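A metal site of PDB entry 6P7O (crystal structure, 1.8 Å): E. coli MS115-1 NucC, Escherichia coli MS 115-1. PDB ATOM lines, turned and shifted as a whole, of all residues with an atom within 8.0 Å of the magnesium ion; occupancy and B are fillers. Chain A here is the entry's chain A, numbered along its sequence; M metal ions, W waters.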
ATOM      1  N   GLY A  35     -20.250  -0.996   9.256  1.00  0.00           N
ATOM      2  CA  GLY A  35     -19.299  -1.938   9.792  1.00  0.00           C
ATOM      3  C   GLY A  35     -19.614  -2.943   8.738  1.00  0.00           C
ATOM      4  O   GLY A  35     -19.252  -2.697   7.583  1.00  0.00           O
ATOM      5  N   ASP A  36     -20.498  -3.861   9.176  1.00  0.00           N
ATOM      6  CA  ASP A  36     -20.751  -5.169   8.575  1.00  0.00           C
ATOM      7  C   ASP A  36     -21.040  -5.040   7.096  1.00  0.00           C
ATOM      8  O   ASP A  36     -20.455  -5.784   6.289  1.00  0.00           O
ATOM      9  CB  ASP A  36     -21.924  -5.916   9.290  1.00  0.00           C
ATOM     10  CG  ASP A  36     -21.495  -6.508  10.644  1.00  0.00           C
ATOM     11  OD1 ASP A  36     -20.531  -5.891  11.129  1.00  0.00           O
ATOM     12  OD2 ASP A  36     -22.056  -7.489  11.186  1.00  0.00           O
ATOM     13  N   ALA A  37     -21.867  -4.072   6.688  1.00  0.00           N
ATOM     14  CA  ALA A  37     -22.173  -3.908   5.266  1.00  0.00           C
ATOM     15  C   ALA A  37     -21.817  -2.530   4.708  1.00  0.00           C
ATOM     16  O   ALA A  37     -22.332  -2.151   3.644  1.00  0.00           O
ATOM     17  CB  ALA A  37     -23.657  -4.198   5.015  1.00  0.00           C
ATOM     18  N   SER A  38     -20.946  -1.769   5.370  1.00  0.00           N
ATOM     19  CA  SER A  38     -20.704  -0.401   4.912  1.00  0.00           C
ATOM     20  C   SER A  38     -19.951  -0.368   3.593  1.00  0.00           C
ATOM     21  O   SER A  38     -19.828   0.690   3.011  1.00  0.00           O
ATOM     22  CB  SER A  38     -19.957   0.415   5.968  1.00  0.00           C
ATOM     23  OG  SER A  38     -18.716  -0.141   6.281  1.00  0.00           O
ATOM     24  N   GLU A  39     -19.498  -1.521   3.081  1.00  0.00           N
ATOM     25  CA  GLU A  39     -18.689  -1.462   1.879  1.00  0.00           C
ATOM     26  C   GLU A  39     -19.521  -1.125   0.667  1.00  0.00           C
ATOM     27  O   GLU A  39     -18.963  -0.573  -0.279  1.00  0.00           O
ATOM     28  CB  GLU A  39     -17.922  -2.784   1.599  1.00  0.00           C
ATOM     29  CG  GLU A  39     -18.727  -4.038   1.239  1.00  0.00           C
ATOM     30  CD  GLU A  39     -19.084  -4.888   2.484  1.00  0.00           C
ATOM     31  OE1 GLU A  39     -18.926  -4.404   3.627  1.00  0.00           O
ATOM     32  OE2 GLU A  39     -19.518  -6.052   2.284  1.00  0.00           O
ATOM     33  N   ASN A  58     -17.030  -5.917  -4.546  1.00  0.00           N
ATOM     34  CA  ASN A  58     -16.731  -6.805  -3.424  1.00  0.00           C
ATOM     35  C   ASN A  58     -16.300  -8.153  -3.998  1.00  0.00           C
ATOM     36  O   ASN A  58     -17.027  -8.713  -4.795  1.00  0.00           O
ATOM     37  CB  ASN A  58     -18.006  -6.919  -2.614  1.00  0.00           C
ATOM     38  CG  ASN A  58     -17.908  -7.916  -1.394  1.00  0.00           C
ATOM     39  OD1 ASN A  58     -18.907  -8.572  -1.082  1.00  0.00           O
ATOM     40  ND2 ASN A  58     -16.833  -7.946  -0.716  1.00  0.00           N
ATOM     41  N   GLN A  71     -12.020 -12.457   1.698  1.00  0.00           N
ATOM     42  CA  GLN A  71     -12.981 -11.654   0.965  1.00  0.00           C
ATOM     43  C   GLN A  71     -12.660 -10.172   1.147  1.00  0.00           C
ATOM     44  O   GLN A  71     -12.513  -9.704   2.286  1.00  0.00           O
ATOM     45  CB  GLN A  71     -14.377 -11.931   1.457  1.00  0.00           C
ATOM     46  CG  GLN A  71     -15.428 -11.287   0.534  1.00  0.00           C
ATOM     47  CD  GLN A  71     -16.847 -11.573   1.026  1.00  0.00           C
ATOM     48  OE1 GLN A  71     -17.025 -12.339   1.972  1.00  0.00           O
ATOM     49  NE2 GLN A  71     -17.823 -10.943   0.403  1.00  0.00           N
ATOM     50  N   ILE A  72     -12.573  -9.446   0.045  1.00  0.00           N
ATOM     51  CA  ILE A  72     -12.129  -8.051   0.084  1.00  0.00           C
ATOM     52  C   ILE A  72     -13.322  -7.147  -0.101  1.00  0.00           C
ATOM     53  O   ILE A  72     -14.101  -7.317  -1.060  1.00  0.00           O
ATOM     54  CB  ILE A  72     -11.053  -7.780  -0.944  1.00  0.00           C
ATOM     55  CG1 ILE A  72      -9.850  -8.730  -0.796  1.00  0.00           C
ATOM     56  CG2 ILE A  72     -10.669  -6.317  -0.898  1.00  0.00           C
ATOM     57  CD1 ILE A  72      -9.122  -8.678   0.565  1.00  0.00           C
ATOM     58  N   ASP A  73     -13.533  -6.222   0.849  1.00  0.00           N
ATOM     59  CA  ASP A  73     -14.716  -5.377   0.754  1.00  0.00           C
ATOM     60  C   ASP A  73     -14.758  -4.609  -0.564  1.00  0.00           C
ATOM     61  O   ASP A  73     -15.836  -4.476  -1.151  1.00  0.00           O
ATOM     62  CB  ASP A  73     -14.804  -4.389   1.964  1.00  0.00           C
ATOM     63  CG  ASP A  73     -15.040  -5.027   3.229  1.00  0.00           C
ATOM     64  OD1 ASP A  73     -15.296  -6.237   3.305  1.00  0.00           O
ATOM     65  OD2 ASP A  73     -15.009  -4.308   4.275  1.00  0.00           O
ATOM     66  N   VAL A  74     -13.673  -3.988  -0.974  1.00  0.00           N
ATOM     67  CA  VAL A  74     -13.612  -3.199  -2.184  1.00  0.00           C
ATOM     68  C   VAL A  74     -12.359  -3.562  -2.964  1.00  0.00           C
ATOM     69  O   VAL A  74     -11.261  -3.207  -2.533  1.00  0.00           O
ATOM     70  CB  VAL A  74     -13.617  -1.694  -1.913  1.00  0.00           C
ATOM     71  CG1 VAL A  74     -13.705  -1.021  -3.224  1.00  0.00           C
ATOM     72  CG2 VAL A  74     -14.733  -1.308  -1.032  1.00  0.00           C
ATOM     73  N   PHE A 103      -9.454  -2.475  -0.487  1.00  0.00           N
ATOM     74  CA  PHE A 103      -9.826  -1.736   0.723  1.00  0.00           C
ATOM     75  C   PHE A 103     -10.687  -2.569   1.651  1.00  0.00           C
ATOM     76  O   PHE A 103     -11.521  -3.330   1.199  1.00  0.00           O
ATOM     77  CB  PHE A 103     -10.603  -0.420   0.390  1.00  0.00           C
ATOM     78  CG  PHE A 103      -9.785   0.517  -0.479  1.00  0.00           C
ATOM     79  CD1 PHE A 103      -8.909   1.389   0.097  1.00  0.00           C
ATOM     80  CD2 PHE A 103      -9.846   0.457  -1.835  1.00  0.00           C
ATOM     81  CE1 PHE A 103      -8.091   2.217  -0.616  1.00  0.00           C
ATOM     82  CE2 PHE A 103      -9.017   1.312  -2.624  1.00  0.00           C
ATOM     83  CZ  PHE A 103      -8.165   2.189  -2.049  1.00  0.00           C
ATOM     84  N   GLU A 104     -10.560  -2.298   2.944  1.00  0.00           N
ATOM     85  CA  GLU A 104     -11.438  -2.855   3.974  1.00  0.00           C
ATOM     86  C   GLU A 104     -12.290  -1.689   4.483  1.00  0.00           C
ATOM     87  O   GLU A 104     -11.763  -0.606   4.726  1.00  0.00           O
ATOM     88  CB  GLU A 104     -10.629  -3.452   5.129  1.00  0.00           C
ATOM     89  CG  GLU A 104     -11.497  -3.801   6.382  1.00  0.00           C
ATOM     90  CD  GLU A 104     -12.560  -4.813   6.061  1.00  0.00           C
ATOM     91  OE1 GLU A 104     -12.284  -5.667   5.184  1.00  0.00           O
ATOM     92  OE2 GLU A 104     -13.674  -4.783   6.716  1.00  0.00           O
ATOM     93  N   ALA A 105     -13.581  -1.911   4.607  1.00  0.00           N
ATOM     94  CA  ALA A 105     -14.550  -0.907   5.092  1.00  0.00           C
ATOM     95  C   ALA A 105     -15.207  -1.349   6.395  1.00  0.00           C
ATOM     96  O   ALA A 105     -15.556  -2.518   6.566  1.00  0.00           O
ATOM     97  CB  ALA A 105     -15.649  -0.667   4.056  1.00  0.00           C
ATOM     98  N   LYS A 106     -15.470  -0.393   7.281  1.00  0.00           N
ATOM     99  CA  LYS A 106     -16.244  -0.634   8.494  1.00  0.00           C
ATOM    100  C   LYS A 106     -16.687   0.741   9.004  1.00  0.00           C
ATOM    101  O   LYS A 106     -16.117   1.761   8.654  1.00  0.00           O
ATOM    102  CB  LYS A 106     -15.451  -1.362   9.574  1.00  0.00           C
ATOM    103  CG  LYS A 106     -16.321  -2.068  10.610  1.00  0.00           C
ATOM    104  CD  LYS A 106     -15.521  -2.615  11.880  1.00  0.00           C
ATOM    105  CE  LYS A 106     -16.318  -3.500  12.868  1.00  0.00           C
ATOM    106  NZ  LYS A 106     -15.572  -3.524  14.233  1.00  0.00           N
ATOM    107  N   GLN A 107     -17.719   0.748   9.837  1.00  0.00           N
ATOM    108  CA  GLN A 107     -18.314   2.003  10.223  1.00  0.00           C
ATOM    109  C   GLN A 107     -17.280   2.856  10.949  1.00  0.00           C
ATOM    110  O   GLN A 107     -17.149   4.056  10.697  1.00  0.00           O
ATOM    111  CB  GLN A 107     -19.494   1.739  11.140  1.00  0.00           C
ATOM    112  CG  GLN A 107     -20.037   2.971  11.824  1.00  0.00           C
ATOM    113  CD  GLN A 107     -20.738   3.942  10.861  1.00  0.00           C
ATOM    114  OE1 GLN A 107     -21.146   3.553   9.761  1.00  0.00           O
ATOM    115  NE2 GLN A 107     -20.883   5.213  11.284  1.00  0.00           N
ATOM    116  N   LEU A 113      -9.725  -2.973  13.735  1.00  0.00           N
ATOM    117  CA  LEU A 113     -10.058  -2.862  12.303  1.00  0.00           C
ATOM    118  C   LEU A 113      -8.826  -2.592  11.457  1.00  0.00           C
ATOM    119  O   LEU A 113      -8.668  -3.168  10.360  1.00  0.00           O
ATOM    120  CB  LEU A 113     -11.095  -1.763  12.103  1.00  0.00           C
ATOM    121  CG  LEU A 113     -11.332  -1.460  10.602  1.00  0.00           C
ATOM    122  CD1 LEU A 113     -11.967  -2.588   9.902  1.00  0.00           C
ATOM    123  CD2 LEU A 113     -12.241  -0.314  10.531  1.00  0.00           C
ATOM    124  N   TYR A 116      -7.016  -5.840  11.047  1.00  0.00           N
ATOM    125  CA  TYR A 116      -7.807  -6.682  10.151  1.00  0.00           C
ATOM    126  C   TYR A 116      -7.633  -6.242   8.714  1.00  0.00           C
ATOM    127  O   TYR A 116      -7.472  -7.089   7.845  1.00  0.00           O
ATOM    128  CB  TYR A 116      -9.248  -6.581  10.598  1.00  0.00           C
ATOM    129  CG  TYR A 116     -10.252  -7.396   9.929  1.00  0.00           C
ATOM    130  CD1 TYR A 116     -10.119  -8.768   9.847  1.00  0.00           C
ATOM    131  CD2 TYR A 116     -11.367  -6.801   9.338  1.00  0.00           C
ATOM    132  CE1 TYR A 116     -11.112  -9.597   9.286  1.00  0.00           C
ATOM    133  CE2 TYR A 116     -12.356  -7.584   8.742  1.00  0.00           C
ATOM    134  CZ  TYR A 116     -12.231  -8.981   8.759  1.00  0.00           C
ATOM    135  OH  TYR A 116     -13.152  -9.746   8.151  1.00  0.00           O
ATOM    136  N   LYS A 120      -6.074  -8.599   5.639  1.00  0.00           N
ATOM    137  CA  LYS A 120      -6.732  -8.754   4.323  1.00  0.00           C
ATOM    138  C   LYS A 120      -5.837  -8.345   3.191  1.00  0.00           C
ATOM    139  O   LYS A 120      -5.755  -9.053   2.168  1.00  0.00           O
ATOM    140  CB  LYS A 120      -8.030  -7.960   4.298  1.00  0.00           C
ATOM    141  CG  LYS A 120      -9.094  -8.610   5.150  1.00  0.00           C
ATOM    142  CD  LYS A 120     -10.330  -8.618   4.438  1.00  0.00           C
ATOM    143  CE  LYS A 120     -11.428  -8.868   5.362  1.00  0.00           C
ATOM    144  NZ  LYS A 120     -12.685  -8.430   4.747  1.00  0.00           N
ATOM    145  N   LEU A 154     -11.473   2.186   4.822  1.00  0.00           N
ATOM    146  CA  LEU A 154     -12.513   3.177   4.562  1.00  0.00           C
ATOM    147  C   LEU A 154     -13.511   3.105   5.714  1.00  0.00           C
ATOM    148  O   LEU A 154     -14.125   2.057   5.919  1.00  0.00           O
ATOM    149  CB  LEU A 154     -13.223   2.859   3.234  1.00  0.00           C
ATOM    150  CG  LEU A 154     -12.295   2.871   1.984  1.00  0.00           C
ATOM    151  CD1 LEU A 154     -13.107   2.265   0.764  1.00  0.00           C
ATOM    152  CD2 LEU A 154     -11.781   4.234   1.733  1.00  0.00           C
HETATM  153 MG    MG M   1     -15.531  -4.566   6.229  1.00  0.00          MG
HETATM  154  O   HOH W   1     -17.389  -4.283   5.870  1.00  0.00           O
HETATM  155  O   HOH W   2     -15.895  -6.625   5.861  1.00  0.00           O
HETATM  156  O   HOH W   3     -16.265  -4.907   8.216  1.00  0.00           O
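OD1 of Asp 73 lies within salt-bridge range of NZ of Lys 120.
The backbone carbonyl oxygen of Glu 104 lies within hydrogen-bond range of the backbone NH of Leu 154 (2.8 Å).
The side-chain amino group (NZ) of Lys 120 is in salt-bridge range of the side-chain carboxylate (OE1) of Glu 104 (2.8 Å).
Three residues have an atom within 4 Å of the magnesium ion: Asp 73, Glu 104 and Ala 105.
Along chain A the residues within 4 Å of the magnesium ion span positions 73 to 105.
The nearest printed residue that does not touch the magnesium ion is Glu 39 (4.3 Å).
The magnesium ion is bound by water W1 (1.9 Å), OE2 of Glu 104 (1.9 Å), OD2 of Asp 73 (2.0 Å), O of Ala 105 (2.1 Å), water W2 (2.1 Å) and water W3 (2.1 Å).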
